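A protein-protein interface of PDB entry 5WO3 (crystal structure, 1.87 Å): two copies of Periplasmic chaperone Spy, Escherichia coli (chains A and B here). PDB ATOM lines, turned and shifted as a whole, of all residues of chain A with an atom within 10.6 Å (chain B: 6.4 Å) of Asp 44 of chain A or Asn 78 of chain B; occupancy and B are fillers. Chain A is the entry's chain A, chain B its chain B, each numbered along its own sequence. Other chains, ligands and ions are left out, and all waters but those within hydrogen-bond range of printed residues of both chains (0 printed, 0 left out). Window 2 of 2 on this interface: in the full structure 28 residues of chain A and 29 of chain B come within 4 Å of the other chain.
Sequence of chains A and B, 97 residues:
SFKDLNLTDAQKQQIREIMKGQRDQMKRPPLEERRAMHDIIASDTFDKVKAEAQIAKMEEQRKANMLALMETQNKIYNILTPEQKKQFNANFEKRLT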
ATOM      1  N   HIS A  38     -34.873 -16.617 -21.742  1.00  0.00           N
ATOM      2  CA  HIS A  38     -34.735 -15.514 -20.812  1.00  0.00           C
ATOM      3  C   HIS A  38     -34.002 -15.983 -19.537  1.00  0.00           C
ATOM      4  O   HIS A  38     -33.060 -15.340 -19.074  1.00  0.00           O
ATOM      5  CB  HIS A  38     -36.086 -14.937 -20.456  1.00  0.00           C
ATOM      6  CG  HIS A  38     -35.996 -13.617 -19.777  1.00  0.00           C
ATOM      7  ND1 HIS A  38     -37.095 -12.841 -19.501  1.00  0.00           N
ATOM      8  CD2 HIS A  38     -34.921 -12.940 -19.305  1.00  0.00           C
ATOM      9  CE1 HIS A  38     -36.705 -11.743 -18.878  1.00  0.00           C
ATOM     10  NE2 HIS A  38     -35.387 -11.777 -18.759  1.00  0.00           N
ATOM     11  N   ASP A  39     -34.447 -17.105 -18.980  1.00  0.00           N
ATOM     12  CA  ASP A  39     -33.790 -17.728 -17.812  1.00  0.00           C
ATOM     13  C   ASP A  39     -32.306 -18.002 -17.993  1.00  0.00           C
ATOM     14  O   ASP A  39     -31.561 -17.947 -17.041  1.00  0.00           O
ATOM     15  CB  ASP A  39     -34.464 -19.050 -17.475  1.00  0.00           C
ATOM     16  CG  ASP A  39     -35.744 -18.864 -16.737  1.00  0.00           C
ATOM     17  OD1 ASP A  39     -36.012 -17.717 -16.313  1.00  0.00           O
ATOM     18  OD2 ASP A  39     -36.455 -19.880 -16.583  1.00  0.00           O
ATOM     19  N   ILE A  40     -31.893 -18.315 -19.207  1.00  0.00           N
ATOM     20  CA  ILE A  40     -30.494 -18.636 -19.463  1.00  0.00           C
ATOM     21  C   ILE A  40     -29.699 -17.371 -19.540  1.00  0.00           C
ATOM     22  O   ILE A  40     -28.607 -17.247 -18.969  1.00  0.00           O
ATOM     23  CB  ILE A  40     -30.344 -19.434 -20.756  1.00  0.00           C
ATOM     24  CG1 ILE A  40     -30.948 -20.824 -20.545  1.00  0.00           C
ATOM     25  CG2 ILE A  40     -28.859 -19.582 -21.184  1.00  0.00           C
ATOM     26  CD1 ILE A  40     -31.300 -21.499 -21.804  1.00  0.00           C
ATOM     27  N   ILE A  41     -30.278 -16.385 -20.192  1.00  0.00           N
ATOM     28  CA  ILE A  41     -29.606 -15.129 -20.367  1.00  0.00           C
ATOM     29  C   ILE A  41     -29.436 -14.365 -19.047  1.00  0.00           C
ATOM     30  O   ILE A  41     -28.334 -13.887 -18.749  1.00  0.00           O
ATOM     31  CB  ILE A  41     -30.359 -14.261 -21.397  1.00  0.00           C
ATOM     32  CG1 ILE A  41     -30.151 -14.846 -22.809  1.00  0.00           C
ATOM     33  CG2 ILE A  41     -29.843 -12.864 -21.324  1.00  0.00           C
ATOM     34  CD1 ILE A  41     -31.106 -14.291 -23.860  1.00  0.00           C
ATOM     35  N   ALA A  42     -30.496 -14.243 -18.253  1.00  0.00           N
ATOM     36  CA  ALA A  42     -30.455 -13.468 -17.014  1.00  0.00           C
ATOM     37  C   ALA A  42     -29.969 -14.285 -15.766  1.00  0.00           C
ATOM     38  O   ALA A  42     -30.603 -14.268 -14.721  1.00  0.00           O
ATOM     39  CB  ALA A  42     -31.861 -12.851 -16.731  1.00  0.00           C
ATOM     40  N   SER A  43     -28.856 -14.993 -15.912  1.00  0.00           N
ATOM     41  CA  SER A  43     -28.241 -15.747 -14.820  1.00  0.00           C
ATOM     42  C   SER A  43     -26.838 -15.191 -14.616  1.00  0.00           C
ATOM     43  O   SER A  43     -26.334 -14.555 -15.541  1.00  0.00           O
ATOM     44  CB  SER A  43     -28.201 -17.223 -15.158  1.00  0.00           C
ATOM     45  OG  SER A  43     -27.357 -17.880 -14.229  1.00  0.00           O
ATOM     46  N   ASP A  44     -26.180 -15.383 -13.460  1.00  0.00           N
ATOM     47  CA  ASP A  44     -24.876 -14.714 -13.321  1.00  0.00           C
ATOM     48  C   ASP A  44     -23.745 -15.583 -13.942  1.00  0.00           C
ATOM     49  O   ASP A  44     -22.567 -15.202 -13.933  1.00  0.00           O
ATOM     50  CB  ASP A  44     -24.580 -14.305 -11.854  1.00  0.00           C
ATOM     51  CG  ASP A  44     -24.397 -15.479 -10.912  1.00  0.00           C
ATOM     52  OD1 ASP A  44     -24.086 -15.234  -9.706  1.00  0.00           O
ATOM     53  OD2 ASP A  44     -24.548 -16.634 -11.367  1.00  0.00           O
ATOM     54  N   THR A  45     -24.120 -16.738 -14.493  1.00  0.00           N
ATOM     55  CA  THR A  45     -23.214 -17.540 -15.335  1.00  0.00           C
ATOM     56  C   THR A  45     -23.936 -18.046 -16.561  1.00  0.00           C
ATOM     57  O   THR A  45     -25.151 -18.103 -16.557  1.00  0.00           O
ATOM     58  CB  THR A  45     -22.670 -18.748 -14.596  1.00  0.00           C
ATOM     59  OG1 THR A  45     -23.747 -19.667 -14.375  1.00  0.00           O
ATOM     60  CG2 THR A  45     -22.083 -18.333 -13.280  1.00  0.00           C
ATOM     61  N   PHE A  46     -23.187 -18.403 -17.596  1.00  0.00           N
ATOM     62  CA  PHE A  46     -23.764 -19.045 -18.782  1.00  0.00           C
ATOM     63  C   PHE A  46     -23.621 -20.555 -18.675  1.00  0.00           C
ATOM     64  O   PHE A  46     -22.518 -21.102 -18.591  1.00  0.00           O
ATOM     65  CB  PHE A  46     -23.108 -18.536 -20.047  1.00  0.00           C
ATOM     66  CG  PHE A  46     -23.637 -19.188 -21.299  1.00  0.00           C
ATOM     67  CD1 PHE A  46     -24.932 -18.970 -21.704  1.00  0.00           C
ATOM     68  CD2 PHE A  46     -22.847 -20.050 -22.028  1.00  0.00           C
ATOM     69  CE1 PHE A  46     -25.431 -19.574 -22.864  1.00  0.00           C
ATOM     70  CE2 PHE A  46     -23.340 -20.663 -23.162  1.00  0.00           C
ATOM     71  CZ  PHE A  46     -24.633 -20.425 -23.564  1.00  0.00           C
ATOM     72  N   ASP A  47     -24.767 -21.209 -18.621  1.00  0.00           N
ATOM     73  CA  ASP A  47     -24.852 -22.658 -18.458  1.00  0.00           C
ATOM     74  C   ASP A  47     -25.029 -23.321 -19.824  1.00  0.00           C
ATOM     75  O   ASP A  47     -26.131 -23.434 -20.307  1.00  0.00           O
ATOM     76  CB  ASP A  47     -26.014 -22.980 -17.540  1.00  0.00           C
ATOM     77  CG  ASP A  47     -26.054 -24.439 -17.084  1.00  0.00           C
ATOM     78  OD1 ASP A  47     -25.689 -25.349 -17.836  1.00  0.00           O
ATOM     79  OD2 ASP A  47     -26.499 -24.665 -15.950  1.00  0.00           O
ATOM     80  N   LYS A  48     -23.933 -23.735 -20.430  1.00  0.00           N
ATOM     81  CA  LYS A  48     -23.962 -24.226 -21.795  1.00  0.00           C
ATOM     82  C   LYS A  48     -24.757 -25.523 -21.883  1.00  0.00           C
ATOM     83  O   LYS A  48     -25.460 -25.775 -22.866  1.00  0.00           O
ATOM     84  CB  LYS A  48     -22.521 -24.402 -22.310  1.00  0.00           C
ATOM     85  CG  LYS A  48     -22.383 -25.162 -23.640  1.00  0.00           C
ATOM     86  CD  LYS A  48     -20.927 -25.184 -24.108  1.00  0.00           C
ATOM     87  CE  LYS A  48     -20.495 -26.550 -24.638  1.00  0.00           C
ATOM     88  NZ  LYS A  48     -21.091 -26.882 -25.973  1.00  0.00           N
ATOM     89  N   GLN B  73     -25.521 -12.464 -24.985  1.00  0.00           N
ATOM     90  CA  GLN B  73     -26.482 -11.705 -24.187  1.00  0.00           C
ATOM     91  C   GLN B  73     -26.255 -11.884 -22.669  1.00  0.00           C
ATOM     92  O   GLN B  73     -26.425 -10.965 -21.888  1.00  0.00           O
ATOM     93  CB  GLN B  73     -27.894 -12.116 -24.550  1.00  0.00           C
ATOM     94  CG  GLN B  73     -28.264 -11.727 -25.978  1.00  0.00           C
ATOM     95  CD  GLN B  73     -28.440 -10.240 -26.139  1.00  0.00           C
ATOM     96  OE1 GLN B  73     -29.359  -9.652 -25.574  1.00  0.00           O
ATOM     97  NE2 GLN B  73     -27.561  -9.619 -26.917  1.00  0.00           N
ATOM     98  N   ASN B  74     -25.908 -13.100 -22.270  1.00  0.00           N
ATOM     99  CA  ASN B  74     -25.623 -13.384 -20.872  1.00  0.00           C
ATOM    100  C   ASN B  74     -24.435 -12.558 -20.395  1.00  0.00           C
ATOM    101  O   ASN B  74     -24.425 -12.016 -19.280  1.00  0.00           O
ATOM    102  CB  ASN B  74     -25.367 -14.874 -20.702  1.00  0.00           C
ATOM    103  CG  ASN B  74     -25.019 -15.223 -19.289  1.00  0.00           C
ATOM    104  OD1 ASN B  74     -23.882 -15.061 -18.876  1.00  0.00           O
ATOM    105  ND2 ASN B  74     -26.000 -15.651 -18.523  1.00  0.00           N
ATOM    106  N   LYS B  75     -23.421 -12.464 -21.246  1.00  0.00           N
ATOM    107  CA  LYS B  75     -22.218 -11.713 -20.905  1.00  0.00           C
ATOM    108  C   LYS B  75     -22.610 -10.238 -20.742  1.00  0.00           C
ATOM    109  O   LYS B  75     -22.105  -9.524 -19.880  1.00  0.00           O
ATOM    110  CB  LYS B  75     -21.145 -11.874 -21.980  1.00  0.00           C
ATOM    111  CG  LYS B  75     -20.319 -13.177 -21.908  1.00  0.00           C
ATOM    112  CD  LYS B  75     -19.323 -13.215 -23.066  1.00  0.00           C
ATOM    113  CE  LYS B  75     -18.119 -14.111 -22.812  1.00  0.00           C
ATOM    114  NZ  LYS B  75     -18.381 -15.545 -23.035  1.00  0.00           N
ATOM    115  N   ILE B  76     -23.513  -9.777 -21.585  1.00  0.00           N
ATOM    116  CA  ILE B  76     -23.911  -8.355 -21.499  1.00  0.00           C
ATOM    117  C   ILE B  76     -24.726  -8.118 -20.228  1.00  0.00           C
ATOM    118  O   ILE B  76     -24.524  -7.135 -19.497  1.00  0.00           O
ATOM    119  CB  ILE B  76     -24.705  -7.935 -22.746  1.00  0.00           C
ATOM    120  CG1 ILE B  76     -23.784  -7.974 -23.978  1.00  0.00           C
ATOM    121  CG2 ILE B  76     -25.345  -6.527 -22.547  1.00  0.00           C
ATOM    122  CD1 ILE B  76     -24.481  -7.779 -25.307  1.00  0.00           C
ATOM    123  N   TYR B  77     -25.655  -9.022 -19.965  1.00  0.00           N
ATOM    124  CA  TYR B  77     -26.493  -8.914 -18.794  1.00  0.00           C
ATOM    125  C   TYR B  77     -25.613  -8.728 -17.564  1.00  0.00           C
ATOM    126  O   TYR B  77     -25.889  -7.903 -16.710  1.00  0.00           O
ATOM    127  CB  TYR B  77     -27.355 -10.160 -18.644  1.00  0.00           C
ATOM    128  CG  TYR B  77     -28.362 -10.072 -17.540  1.00  0.00           C
ATOM    129  CD1 TYR B  77     -29.551  -9.403 -17.726  1.00  0.00           C
ATOM    130  CD2 TYR B  77     -28.116 -10.650 -16.309  1.00  0.00           C
ATOM    131  CE1 TYR B  77     -30.475  -9.299 -16.717  1.00  0.00           C
ATOM    132  CE2 TYR B  77     -29.030 -10.556 -15.279  1.00  0.00           C
ATOM    133  CZ  TYR B  77     -30.213  -9.882 -15.494  1.00  0.00           C
ATOM    134  OH  TYR B  77     -31.136  -9.816 -14.498  1.00  0.00           O
ATOM    135  N   ASN B  78     -24.510  -9.474 -17.511  1.00  0.00           N
ATOM    136  CA  ASN B  78     -23.691  -9.497 -16.300  1.00  0.00           C
ATOM    137  C   ASN B  78     -22.658  -8.389 -16.174  1.00  0.00           C
ATOM    138  O   ASN B  78     -21.893  -8.392 -15.219  1.00  0.00           O
ATOM    139  CB  ASN B  78     -23.010 -10.855 -16.172  1.00  0.00           C
ATOM    140  CG  ASN B  78     -23.954 -11.884 -15.633  1.00  0.00           C
ATOM    141  OD1 ASN B  78     -24.359 -11.800 -14.464  1.00  0.00           O
ATOM    142  ND2 ASN B  78     -24.399 -12.806 -16.490  1.00  0.00           N
ATOM    143  N   ILE B  79     -22.637  -7.434 -17.101  1.00  0.00           N
ATOM    144  CA  ILE B  79     -21.921  -6.192 -16.827  1.00  0.00           C
ATOM    145  C   ILE B  79     -22.867  -5.060 -16.475  1.00  0.00           C
ATOM    146  O   ILE B  79     -22.425  -3.945 -16.342  1.00  0.00           O
ATOM    147  CB  ILE B  79     -21.048  -5.744 -18.008  1.00  0.00           C
ATOM    148  CG1 ILE B  79     -21.892  -5.367 -19.209  1.00  0.00           C
ATOM    149  CG2 ILE B  79     -20.059  -6.822 -18.363  1.00  0.00           C
ATOM    150  CD1 ILE B  79     -21.170  -4.528 -20.193  1.00  0.00           C
ATOM    151  N   LEU B  80     -24.163  -5.329 -16.342  1.00  0.00           N
ATOM    152  CA  LEU B  80     -25.146  -4.270 -16.049  1.00  0.00           C
ATOM    153  C   LEU B  80     -25.313  -4.091 -14.562  1.00  0.00           C
ATOM    154  O   LEU B  80     -25.093  -5.029 -13.828  1.00  0.00           O
ATOM    155  CB  LEU B  80     -26.525  -4.608 -16.655  1.00  0.00           C
ATOM    156  CG  LEU B  80     -26.667  -4.861 -18.135  1.00  0.00           C
ATOM    157  CD1 LEU B  80     -28.166  -5.104 -18.583  1.00  0.00           C
ATOM    158  CD2 LEU B  80     -26.078  -3.687 -18.841  1.00  0.00           C
ATOM    159  N   LYS B  85     -30.344  -3.990 -15.128  1.00  0.00           N
ATOM    160  CA  LYS B  85     -30.839  -5.343 -15.398  1.00  0.00           C
ATOM    161  C   LYS B  85     -32.360  -5.415 -15.405  1.00  0.00           C
ATOM    162  O   LYS B  85     -32.945  -6.184 -16.167  1.00  0.00           O
ATOM    163  CB  LYS B  85     -30.299  -6.348 -14.377  1.00  0.00           C
ATOM    164  CG  LYS B  85     -28.795  -6.662 -14.482  1.00  0.00           C
ATOM    165  CD  LYS B  85     -28.324  -7.640 -13.389  1.00  0.00           C
ATOM    166  CE  LYS B  85     -26.816  -7.827 -13.433  1.00  0.00           C
ATOM    167  NZ  LYS B  85     -26.294  -8.649 -12.331  1.00  0.00           N
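No position is printed for both chains.
Hydrophobic or aromatic side chains of chain B that line the printed part of chain A: Tyr 77. Of the 11 printed residues of chain A, 7 touch a printed residue of chain B. Among the printed residues, 10 pairs touch across the chains.
His 38 of chain A touches none of the printed residues of chain B. Of the printed residues of chain B, Ile 40 of chain A touches Asn 74. Of the printed residues of chain B, Ile 41 of chain A touches Gln 73, Asn 74 and Tyr 77. Printed residues of chain B within 4 Å of Ala 42 of chain A: Tyr 77 (3.6 Å). Of the printed residues of chain B, Ser 43 of chain A touches Asn 74 (3.2 Å) and Asn 78 (2.8 Å). Of chain B, only Asn 78 comes within 4 Å of Asp 44 of chain A. Of the printed residues of chain B, Thr 45 of chain A touches Asn 74 (3.3 Å). Asp 47 of chain A touches none of the printed residues of chain B. Asn 78 of chain B touches two residues of chain A. No residue of chain A comes within 4 Å of Ile 79 of chain B. The nearest residue of chain B that does not touch Asp 44 of chain A is Asn 74 of chain B (5.0 Å).
The side-chain hydroxyl of Ser 43 of chain A is in hydrogen-bond range of the backbone carbonyl oxygen of Thr 45 of chain A (3.2 Å). The backbone carbonyl oxygen (O) of Asn 74 of chain B is in hydrogen-bond range of the side-chain amide nitrogen (ND2) of Asn 78 of chain B (2.9 Å).
Among the printed residues, merely in contact across the chains: Ile 41 of chain A with Gln 73 of chain B (3.8 Å), Ile 41 of chain A with Tyr 77 of chain B (3.9 Å), Ala 42 of chain A with Tyr 77 of chain B (3.6 Å), Asp 44 of chain A with Asn 78 of chain B (3.2 Å) and Phe 46 of chain A with Asn 74 of chain B (3.6 Å).
O of Ile 40 of chain A lies within hydrogen-bond range of ND2 of Asn 74 of chain B, at 3.1 Å. O of Ile 41 of chain A lies within hydrogen-bond range of ND2 of Asn 74 of chain B (2.9 Å). O of Ser 43 of chain A sits at hydrogen-bond distance from ND2 of Asn 74 of chain B (3.2 Å). O of Ser 43 of chain A sits at hydrogen-bond distance from ND2 of Asn 78 of chain B, at 2.8 Å. The backbone carbonyl oxygen of Thr 45 of chain A lies within hydrogen-bond range of the side-chain amide nitrogen of Asn 74 of chain B (3.3 Å).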
